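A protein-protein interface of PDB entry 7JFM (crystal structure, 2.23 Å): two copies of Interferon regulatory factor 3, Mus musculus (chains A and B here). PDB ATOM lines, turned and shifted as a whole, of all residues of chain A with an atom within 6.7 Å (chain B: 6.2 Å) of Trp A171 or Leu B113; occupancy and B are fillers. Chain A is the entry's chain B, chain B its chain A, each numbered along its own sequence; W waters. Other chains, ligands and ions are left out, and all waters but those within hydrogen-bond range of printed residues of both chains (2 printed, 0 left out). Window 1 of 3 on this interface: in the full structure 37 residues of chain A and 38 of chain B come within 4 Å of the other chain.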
ATOM      1  N   PHE A  23      13.909  21.477 -29.477  1.00  0.00           N
ATOM      2  CA  PHE A  23      14.357  22.063 -28.221  1.00  0.00           C
ATOM      3  C   PHE A  23      13.650  23.392 -28.003  1.00  0.00           C
ATOM      4  O   PHE A  23      13.670  24.258 -28.882  1.00  0.00           O
ATOM      5  CB  PHE A  23      15.877  22.273 -28.212  1.00  0.00           C
ATOM      6  CG  PHE A  23      16.671  21.013 -28.421  1.00  0.00           C
ATOM      7  CD1 PHE A  23      16.954  20.562 -29.700  1.00  0.00           C
ATOM      8  CD2 PHE A  23      17.143  20.289 -27.340  1.00  0.00           C
ATOM      9  CE1 PHE A  23      17.688  19.405 -29.896  1.00  0.00           C
ATOM     10  CE2 PHE A  23      17.878  19.132 -27.529  1.00  0.00           C
ATOM     11  CZ  PHE A  23      18.150  18.689 -28.809  1.00  0.00           C
ATOM     12  N   ARG A  25      13.939  26.522 -25.666  1.00  0.00           N
ATOM     13  CA  ARG A  25      14.764  27.256 -24.705  1.00  0.00           C
ATOM     14  C   ARG A  25      15.763  26.320 -24.022  1.00  0.00           C
ATOM     15  O   ARG A  25      15.900  26.289 -22.797  1.00  0.00           O
ATOM     16  CB  ARG A  25      13.880  27.982 -23.683  1.00  0.00           C
ATOM     17  CG  ARG A  25      14.588  28.998 -22.784  1.00  0.00           C
ATOM     18  CD  ARG A  25      14.909  30.303 -23.497  1.00  0.00           C
ATOM     19  NE  ARG A  25      15.257  31.350 -22.537  1.00  0.00           N
ATOM     20  CZ  ARG A  25      15.662  32.573 -22.868  1.00  0.00           C
ATOM     21  NH1 ARG A  25      15.779  32.913 -24.145  1.00  0.00           N
ATOM     22  NH2 ARG A  25      15.952  33.454 -21.921  1.00  0.00           N
ATOM     23  N   GLY A  26      16.459  25.534 -24.838  1.00  0.00           N
ATOM     24  CA  GLY A  26      17.454  24.616 -24.317  1.00  0.00           C
ATOM     25  C   GLY A  26      16.894  23.446 -23.539  1.00  0.00           C
ATOM     26  O   GLY A  26      17.532  22.980 -22.590  1.00  0.00           O
ATOM     27  N   ARG A  27      15.710  22.960 -23.910  1.00  0.00           N
ATOM     28  CA  ARG A  27      15.118  21.783 -23.286  1.00  0.00           C
ATOM     29  C   ARG A  27      14.584  20.871 -24.376  1.00  0.00           C
ATOM     30  O   ARG A  27      13.761  21.297 -25.192  1.00  0.00           O
ATOM     31  CB  ARG A  27      13.988  22.159 -22.322  1.00  0.00           C
ATOM     32  CG  ARG A  27      14.433  22.691 -20.974  1.00  0.00           C
ATOM     33  CD  ARG A  27      13.319  22.503 -19.956  1.00  0.00           C
ATOM     34  NE  ARG A  27      13.415  23.426 -18.831  1.00  0.00           N
ATOM     35  CZ  ARG A  27      12.515  23.501 -17.856  1.00  0.00           C
ATOM     36  NH1 ARG A  27      11.454  22.705 -17.867  1.00  0.00           N
ATOM     37  NH2 ARG A  27      12.675  24.372 -16.870  1.00  0.00           N
ATOM     38  N   LEU A 112      24.668  17.263 -30.680  1.00  0.00           N
ATOM     39  CA  LEU A 112      24.343  17.876 -29.399  1.00  0.00           C
ATOM     40  C   LEU A 112      24.747  19.342 -29.329  1.00  0.00           C
ATOM     41  O   LEU A 112      24.700  19.933 -28.245  1.00  0.00           O
ATOM     42  CB  LEU A 112      24.995  17.098 -28.250  1.00  0.00           C
ATOM     43  CG  LEU A 112      24.293  15.836 -27.736  1.00  0.00           C
ATOM     44  CD1 LEU A 112      24.361  14.699 -28.745  1.00  0.00           C
ATOM     45  CD2 LEU A 112      24.882  15.403 -26.401  1.00  0.00           C
ATOM     46  N   LEU A 113      25.136  19.946 -30.452  1.00  0.00           N
ATOM     47  CA  LEU A 113      25.593  21.328 -30.445  1.00  0.00           C
ATOM     48  C   LEU A 113      25.600  21.911 -31.852  1.00  0.00           C
ATOM     49  O   LEU A 113      26.393  21.482 -32.700  1.00  0.00           O
ATOM     50  CB  LEU A 113      26.993  21.426 -29.835  1.00  0.00           C
ATOM     51  CG  LEU A 113      27.644  22.810 -29.852  1.00  0.00           C
ATOM     52  CD1 LEU A 113      26.836  23.798 -29.026  1.00  0.00           C
ATOM     53  CD2 LEU A 113      29.076  22.734 -29.353  1.00  0.00           C
ATOM     54  N   PRO A 114      24.733  22.878 -32.144  1.00  0.00           N
ATOM     55  CA  PRO A 114      24.859  23.620 -33.401  1.00  0.00           C
ATOM     56  C   PRO A 114      26.026  24.590 -33.337  1.00  0.00           C
ATOM     57  O   PRO A 114      26.449  25.031 -32.265  1.00  0.00           O
ATOM     58  CB  PRO A 114      23.522  24.358 -33.513  1.00  0.00           C
ATOM     59  CG  PRO A 114      23.083  24.528 -32.099  1.00  0.00           C
ATOM     60  CD  PRO A 114      23.556  23.300 -31.366  1.00  0.00           C
ATOM     61  N   SER A 116      27.681  27.789 -33.238  1.00  0.00           N
ATOM     62  CA  SER A 116      27.369  29.171 -32.907  1.00  0.00           C
ATOM     63  C   SER A 116      28.509  30.133 -33.216  1.00  0.00           C
ATOM     64  O   SER A 116      28.300  31.349 -33.170  1.00  0.00           O
ATOM     65  CB  SER A 116      26.994  29.290 -31.425  1.00  0.00           C
ATOM     66  OG  SER A 116      26.687  30.630 -31.082  1.00  0.00           O
ATOM     67  N   TRP A 158      20.374  21.567 -38.326  1.00  0.00           N
ATOM     68  CA  TRP A 158      19.745  22.360 -37.281  1.00  0.00           C
ATOM     69  C   TRP A 158      18.879  23.441 -37.911  1.00  0.00           C
ATOM     70  O   TRP A 158      19.273  24.064 -38.900  1.00  0.00           O
ATOM     71  CB  TRP A 158      20.792  23.003 -36.367  1.00  0.00           C
ATOM     72  CG  TRP A 158      21.510  22.030 -35.485  1.00  0.00           C
ATOM     73  CD1 TRP A 158      22.657  21.352 -35.776  1.00  0.00           C
ATOM     74  CD2 TRP A 158      21.131  21.631 -34.163  1.00  0.00           C
ATOM     75  NE1 TRP A 158      23.016  20.553 -34.717  1.00  0.00           N
ATOM     76  CE2 TRP A 158      22.095  20.706 -33.714  1.00  0.00           C
ATOM     77  CE3 TRP A 158      20.071  21.965 -33.314  1.00  0.00           C
ATOM     78  CZ2 TRP A 158      22.030  20.111 -32.455  1.00  0.00           C
ATOM     79  CZ3 TRP A 158      20.008  21.373 -32.065  1.00  0.00           C
ATOM     80  CH2 TRP A 158      20.982  20.457 -31.647  1.00  0.00           C
ATOM     81  N   PRO A 166      21.593  31.664 -33.797  1.00  0.00           N
ATOM     82  CA  PRO A 166      22.355  32.042 -32.599  1.00  0.00           C
ATOM     83  C   PRO A 166      23.850  32.127 -32.862  1.00  0.00           C
ATOM     84  O   PRO A 166      24.585  31.158 -32.652  1.00  0.00           O
ATOM     85  CB  PRO A 166      22.021  30.920 -31.606  1.00  0.00           C
ATOM     86  CG  PRO A 166      21.673  29.752 -32.465  1.00  0.00           C
ATOM     87  CD  PRO A 166      20.995  30.322 -33.678  1.00  0.00           C
ATOM     88  N   GLN A 169      26.410  33.541 -29.360  1.00  0.00           N
ATOM     89  CA  GLN A 169      25.536  33.506 -28.195  1.00  0.00           C
ATOM     90  C   GLN A 169      25.068  32.071 -27.999  1.00  0.00           C
ATOM     91  O   GLN A 169      25.010  31.310 -28.969  1.00  0.00           O
ATOM     92  CB  GLN A 169      24.338  34.455 -28.364  1.00  0.00           C
ATOM     93  CG  GLN A 169      23.587  34.313 -29.675  1.00  0.00           C
ATOM     94  CD  GLN A 169      22.414  35.271 -29.772  1.00  0.00           C
ATOM     95  OE1 GLN A 169      22.019  35.682 -30.865  1.00  0.00           O
ATOM     96  NE2 GLN A 169      21.847  35.630 -28.626  1.00  0.00           N
ATOM     97  N   PRO A 170      24.746  31.673 -26.767  1.00  0.00           N
ATOM     98  CA  PRO A 170      24.382  30.268 -26.523  1.00  0.00           C
ATOM     99  C   PRO A 170      23.112  29.879 -27.264  1.00  0.00           C
ATOM    100  O   PRO A 170      22.102  30.586 -27.220  1.00  0.00           O
ATOM    101  CB  PRO A 170      24.194  30.214 -25.001  1.00  0.00           C
ATOM    102  CG  PRO A 170      23.915  31.623 -24.599  1.00  0.00           C
ATOM    103  CD  PRO A 170      24.726  32.470 -25.529  1.00  0.00           C
ATOM    104  N   TRP A 171      23.171  28.733 -27.948  1.00  0.00           N
ATOM    105  CA  TRP A 171      22.035  28.268 -28.734  1.00  0.00           C
ATOM    106  C   TRP A 171      20.859  27.847 -27.863  1.00  0.00           C
ATOM    107  O   TRP A 171      19.734  27.754 -28.367  1.00  0.00           O
ATOM    108  CB  TRP A 171      22.455  27.100 -29.629  1.00  0.00           C
ATOM    109  CG  TRP A 171      22.662  25.809 -28.891  1.00  0.00           C
ATOM    110  CD1 TRP A 171      23.819  25.370 -28.316  1.00  0.00           C
ATOM    111  CD2 TRP A 171      21.685  24.786 -28.658  1.00  0.00           C
ATOM    112  NE1 TRP A 171      23.622  24.139 -27.735  1.00  0.00           N
ATOM    113  CE2 TRP A 171      22.320  23.759 -27.932  1.00  0.00           C
ATOM    114  CE3 TRP A 171      20.335  24.641 -28.992  1.00  0.00           C
ATOM    115  CZ2 TRP A 171      21.652  22.602 -27.533  1.00  0.00           C
ATOM    116  CZ3 TRP A 171      19.673  23.492 -28.596  1.00  0.00           C
ATOM    117  CH2 TRP A 171      20.331  22.488 -27.874  1.00  0.00           C
ATOM    118  N   VAL A 172      21.091  27.589 -26.573  1.00  0.00           N
ATOM    119  CA  VAL A 172      20.011  27.186 -25.680  1.00  0.00           C
ATOM    120  C   VAL A 172      19.080  28.334 -25.327  1.00  0.00           C
ATOM    121  O   VAL A 172      18.021  28.098 -24.737  1.00  0.00           O
ATOM    122  CB  VAL A 172      20.581  26.563 -24.390  1.00  0.00           C
ATOM    123  CG1 VAL A 172      21.352  25.293 -24.712  1.00  0.00           C
ATOM    124  CG2 VAL A 172      21.467  27.563 -23.665  1.00  0.00           C
ATOM    125  N   LYS A 173      19.444  29.569 -25.668  1.00  0.00           N
ATOM    126  CA  LYS A 173      18.562  30.703 -25.432  1.00  0.00           C
ATOM    127  C   LYS A 173      17.553  30.912 -26.553  1.00  0.00           C
ATOM    128  O   LYS A 173      16.608  31.687 -26.376  1.00  0.00           O
ATOM    129  CB  LYS A 173      19.383  31.980 -25.232  1.00  0.00           C
ATOM    130  CG  LYS A 173      20.312  31.928 -24.032  1.00  0.00           C
ATOM    131  CD  LYS A 173      19.549  31.580 -22.763  1.00  0.00           C
ATOM    132  CE  LYS A 173      20.486  31.437 -21.575  1.00  0.00           C
ATOM    133  NZ  LYS A 173      19.753  31.057 -20.336  1.00  0.00           N
ATOM    134  N   ARG A 174      17.728  30.244 -27.691  1.00  0.00           N
ATOM    135  CA  ARG A 174      16.761  30.342 -28.774  1.00  0.00           C
ATOM    136  C   ARG A 174      15.456  29.655 -28.390  1.00  0.00           C
ATOM    137  O   ARG A 174      15.437  28.685 -27.628  1.00  0.00           O
ATOM    138  CB  ARG A 174      17.327  29.730 -30.055  1.00  0.00           C
ATOM    139  CG  ARG A 174      18.274  30.651 -30.807  1.00  0.00           C
ATOM    140  CD  ARG A 174      17.551  31.910 -31.259  1.00  0.00           C
ATOM    141  NE  ARG A 174      18.441  32.855 -31.927  1.00  0.00           N
ATOM    142  CZ  ARG A 174      19.065  33.854 -31.312  1.00  0.00           C
ATOM    143  NH1 ARG A 174      18.899  34.042 -30.010  1.00  0.00           N
ATOM    144  NH2 ARG A 174      19.857  34.668 -31.999  1.00  0.00           N
ATOM    145  N   LEU A 175      14.353  30.174 -28.932  1.00  0.00           N
ATOM    146  CA  LEU A 175      13.034  29.702 -28.526  1.00  0.00           C
ATOM    147  C   LEU A 175      12.757  28.297 -29.051  1.00  0.00           C
ATOM    148  O   LEU A 175      12.359  27.410 -28.289  1.00  0.00           O
ATOM    149  CB  LEU A 175      11.959  30.679 -29.001  1.00  0.00           C
ATOM    150  CG  LEU A 175      11.965  32.057 -28.336  1.00  0.00           C
ATOM    151  CD1 LEU A 175      11.040  33.010 -29.074  1.00  0.00           C
ATOM    152  CD2 LEU A 175      11.569  31.952 -26.871  1.00  0.00           C
ATOM    153  N   MET A 177      14.498  25.315 -31.482  1.00  0.00           N
ATOM    154  CA  MET A 177      15.581  24.734 -32.265  1.00  0.00           C
ATOM    155  C   MET A 177      15.224  23.292 -32.591  1.00  0.00           C
ATOM    156  O   MET A 177      14.914  22.507 -31.688  1.00  0.00           O
ATOM    157  CB  MET A 177      16.909  24.794 -31.506  1.00  0.00           C
ATOM    158  CG  MET A 177      17.458  26.198 -31.307  1.00  0.00           C
ATOM    159  SD  MET A 177      18.101  26.908 -32.832  1.00  0.00           S
ATOM    160  CE  MET A 177      19.334  25.687 -33.274  1.00  0.00           C
ATOM    161  N   GLY B 109      27.064  26.354 -15.452  1.00  0.00           N
ATOM    162  CA  GLY B 109      26.575  26.595 -16.791  1.00  0.00           C
ATOM    163  C   GLY B 109      25.123  26.207 -16.936  1.00  0.00           C
ATOM    164  O   GLY B 109      24.381  26.129 -15.956  1.00  0.00           O
ATOM    165  N   GLU B 110      24.727  25.971 -18.182  1.00  0.00           N
ATOM    166  CA  GLU B 110      23.367  25.571 -18.498  1.00  0.00           C
ATOM    167  C   GLU B 110      23.238  24.050 -18.448  1.00  0.00           C
ATOM    168  O   GLU B 110      24.225  23.316 -18.364  1.00  0.00           O
ATOM    169  CB  GLU B 110      22.961  26.106 -19.871  1.00  0.00           C
ATOM    170  CG  GLU B 110      23.221  27.595 -20.048  1.00  0.00           C
ATOM    171  CD  GLU B 110      22.460  28.445 -19.050  1.00  0.00           C
ATOM    172  OE1 GLU B 110      21.258  28.181 -18.835  1.00  0.00           O
ATOM    173  OE2 GLU B 110      23.065  29.373 -18.473  1.00  0.00           O
ATOM    174  N   GLU B 111      21.993  23.575 -18.508  1.00  0.00           N
ATOM    175  CA  GLU B 111      21.738  22.147 -18.364  1.00  0.00           C
ATOM    176  C   GLU B 111      22.112  21.359 -19.614  1.00  0.00           C
ATOM    177  O   GLU B 111      22.372  20.156 -19.516  1.00  0.00           O
ATOM    178  CB  GLU B 111      20.268  21.912 -18.009  1.00  0.00           C
ATOM    179  CG  GLU B 111      19.979  20.535 -17.433  1.00  0.00           C
ATOM    180  CD  GLU B 111      18.706  20.504 -16.612  1.00  0.00           C
ATOM    181  OE1 GLU B 111      18.133  21.584 -16.361  1.00  0.00           O
ATOM    182  OE2 GLU B 111      18.280  19.399 -16.215  1.00  0.00           O
ATOM    183  N   LEU B 112      22.149  22.001 -20.781  1.00  0.00           N
ATOM    184  CA  LEU B 112      22.544  21.334 -22.016  1.00  0.00           C
ATOM    185  C   LEU B 112      23.734  22.002 -22.691  1.00  0.00           C
ATOM    186  O   LEU B 112      24.026  21.690 -23.852  1.00  0.00           O
ATOM    187  CB  LEU B 112      21.368  21.267 -22.998  1.00  0.00           C
ATOM    188  CG  LEU B 112      20.352  20.132 -22.839  1.00  0.00           C
ATOM    189  CD1 LEU B 112      19.444  20.353 -21.636  1.00  0.00           C
ATOM    190  CD2 LEU B 112      19.534  19.971 -24.111  1.00  0.00           C
ATOM    191  N   LEU B 113      24.433  22.904 -22.000  1.00  0.00           N
ATOM    192  CA  LEU B 113      25.529  23.624 -22.636  1.00  0.00           C
ATOM    193  C   LEU B 113      26.461  24.254 -21.607  1.00  0.00           C
ATOM    194  O   LEU B 113      26.078  25.213 -20.925  1.00  0.00           O
ATOM    195  CB  LEU B 113      24.981  24.705 -23.569  1.00  0.00           C
ATOM    196  CG  LEU B 113      26.015  25.558 -24.305  1.00  0.00           C
ATOM    197  CD1 LEU B 113      26.847  24.704 -25.248  1.00  0.00           C
ATOM    198  CD2 LEU B 113      25.333  26.687 -25.062  1.00  0.00           C
ATOM    199  N   PRO B 114      27.681  23.747 -21.462  1.00  0.00           N
ATOM    200  CA  PRO B 114      28.694  24.473 -20.695  1.00  0.00           C
ATOM    201  C   PRO B 114      29.256  25.633 -21.501  1.00  0.00           C
ATOM    202  O   PRO B 114      29.312  25.599 -22.733  1.00  0.00           O
ATOM    203  CB  PRO B 114      29.765  23.409 -20.429  1.00  0.00           C
ATOM    204  CG  PRO B 114      29.632  22.465 -21.574  1.00  0.00           C
ATOM    205  CD  PRO B 114      28.165  22.433 -21.920  1.00  0.00           C
ATOM    206  N   ASP B 115      29.669  26.674 -20.785  1.00  0.00           N
ATOM    207  CA  ASP B 115      30.170  27.884 -21.427  1.00  0.00           C
ATOM    208  C   ASP B 115      31.599  27.658 -21.906  1.00  0.00           C
ATOM    209  O   ASP B 115      32.498  27.402 -21.099  1.00  0.00           O
ATOM    210  CB  ASP B 115      30.103  29.067 -20.464  1.00  0.00           C
ATOM    211  CG  ASP B 115      30.387  30.393 -21.146  1.00  0.00           C
ATOM    212  OD1 ASP B 115      30.544  30.409 -22.386  1.00  0.00           O
ATOM    213  OD2 ASP B 115      30.454  31.421 -20.441  1.00  0.00           O
ATOM    214  N   SER B 116      31.805  27.754 -23.220  1.00  0.00           N
ATOM    215  CA  SER B 116      33.128  27.613 -23.812  1.00  0.00           C
ATOM    216  C   SER B 116      33.801  28.950 -24.095  1.00  0.00           C
ATOM    217  O   SER B 116      34.986  28.965 -24.443  1.00  0.00           O
ATOM    218  CB  SER B 116      33.047  26.800 -25.109  1.00  0.00           C
ATOM    219  OG  SER B 116      32.712  25.449 -24.842  1.00  0.00           O
ATOM    220  N   TRP B 158      29.309  21.614 -14.219  1.00  0.00           N
ATOM    221  CA  TRP B 158      29.983  20.867 -15.272  1.00  0.00           C
ATOM    222  C   TRP B 158      31.394  20.505 -14.830  1.00  0.00           C
ATOM    223  O   TRP B 158      32.088  21.316 -14.211  1.00  0.00           O
ATOM    224  CB  TRP B 158      30.036  21.674 -16.572  1.00  0.00           C
ATOM    225  CG  TRP B 158      28.710  21.795 -17.248  1.00  0.00           C
ATOM    226  CD1 TRP B 158      27.808  22.809 -17.110  1.00  0.00           C
ATOM    227  CD2 TRP B 158      28.132  20.865 -18.170  1.00  0.00           C
ATOM    228  NE1 TRP B 158      26.703  22.569 -17.891  1.00  0.00           N
ATOM    229  CE2 TRP B 158      26.876  21.380 -18.552  1.00  0.00           C
ATOM    230  CE3 TRP B 158      28.552  19.646 -18.712  1.00  0.00           C
ATOM    231  CZ2 TRP B 158      26.040  20.721 -19.449  1.00  0.00           C
ATOM    232  CZ3 TRP B 158      27.720  18.991 -19.603  1.00  0.00           C
ATOM    233  CH2 TRP B 158      26.478  19.530 -19.963  1.00  0.00           C
ATOM    234  N   TRP B 171      32.586  22.019 -26.773  1.00  0.00           N
ATOM    235  CA  TRP B 171      32.647  21.154 -25.599  1.00  0.00           C
ATOM    236  C   TRP B 171      32.385  19.698 -25.962  1.00  0.00           C
ATOM    237  O   TRP B 171      32.840  18.790 -25.254  1.00  0.00           O
ATOM    238  CB  TRP B 171      31.653  21.625 -24.535  1.00  0.00           C
ATOM    239  CG  TRP B 171      30.217  21.331 -24.862  1.00  0.00           C
ATOM    240  CD1 TRP B 171      29.333  22.159 -25.494  1.00  0.00           C
ATOM    241  CD2 TRP B 171      29.494  20.129 -24.561  1.00  0.00           C
ATOM    242  NE1 TRP B 171      28.108  21.546 -25.608  1.00  0.00           N
ATOM    243  CE2 TRP B 171      28.182  20.299 -25.045  1.00  0.00           C
ATOM    244  CE3 TRP B 171      29.833  18.925 -23.935  1.00  0.00           C
ATOM    245  CZ2 TRP B 171      27.206  19.311 -24.921  1.00  0.00           C
ATOM    246  CZ3 TRP B 171      28.862  17.945 -23.813  1.00  0.00           C
ATOM    247  CH2 TRP B 171      27.565  18.144 -24.303  1.00  0.00           C
HETATM  248  O   HOH W   1      20.171  23.948 -21.583  1.00  0.00           O
HETATM  249  O   HOH W   2      25.195  21.917 -26.436  1.00  0.00           O
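The backbone carbonyl oxygen of Val A172 sits at hydrogen-bond distance from the backbone NH of Gly A26, 3.0 Å away.
The backbone NH (N) of Phe A23 lies within hydrogen-bond range of the backbone carbonyl oxygen (O) of Met A177.
O of Glu B110 lies within hydrogen-bond range of NE1 of Trp B158 (2.6 Å).
The guanidinium group (NH1) of Arg A25 sits at hydrogen-bond distance from the backbone carbonyl oxygen (O) of Lys A173 (2.7 Å).
Water W2 lies within hydrogen-bond range of the backbone carbonyl oxygen (O) of Leu A112, the backbone carbonyl oxygen (O) of Leu B112, the indole nitrogen (NE1) of Trp A171 and the indole nitrogen (NE1) of Trp B171.
Water W1 lies within hydrogen-bond range of the backbone NH (N) of Leu B112 and the backbone carbonyl oxygen (O) of Gly A26.
Printed residues of chain B within 4 Å of Phe A23: Leu B112.
Of the printed residues of chain B, Leu A113 touches Leu B113 and Trp B171.
Trp A158 touches none of the printed residues of chain B.
Trp A171 touches just one residue of chain B: Leu B113 (3.8 Å).
Of the printed residues of chain A, Leu B113 touches Leu A113 (3.9 Å), Pro A170 (3.7 Å), Trp A171 (3.8 Å) and Val A172 (3.8 Å).
The nearest residue of chain B that does not touch Trp A171 is Leu B112 (4.5 Å).
The nearest residue of chain A that does not touch Leu B113 is Leu A112 (6.0 Å).
The nearest printed residue of chain B that does not touch Lys A173 is Leu B113 (6.6 Å).
Leu A113 touches its own counterpart, Leu B113.
Leu A113 touches Trp B171, and with the chains exchanged Trp A171 touches Leu B113.
6 positions are printed for both chains.
Leu B112 touches Phe A23.
O of Gly A26 touches CD1 of Leu B112 (3.4 Å).
Leu A113 touches Leu B113.
Leu A113 touches Trp B171 (CD2 to CD1, 3.9 Å).
CB of Pro A170 touches CD2 of Leu B113, at 3.7 Å.
Trp A171 touches Leu B113.
CB of Leu B113 touches CG1 of Val A172, 3.8 Å away.
The side-chain amino group (NZ) of Lys A173 is in salt-bridge range of the side-chain carboxylate (OE1) of Glu B110 (3.6 Å).
Of the 18 printed residues of chain A, 7 touch a printed residue of chain B.
Hydrophobic or aromatic side chains of chain A within 4 Å of the printed part of chain B: Phe A23, Leu A113, Pro A170, Trp A171 and Val A172.
Of the 10 printed residues of chain B, 4 touch a printed residue of chain A.
Among the printed residues, Asp or Glu carboxylates within 4 Å of a Lys or Arg side-chain nitrogen of the other chain: Lys A173 with Glu B110 (3.6 Å).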
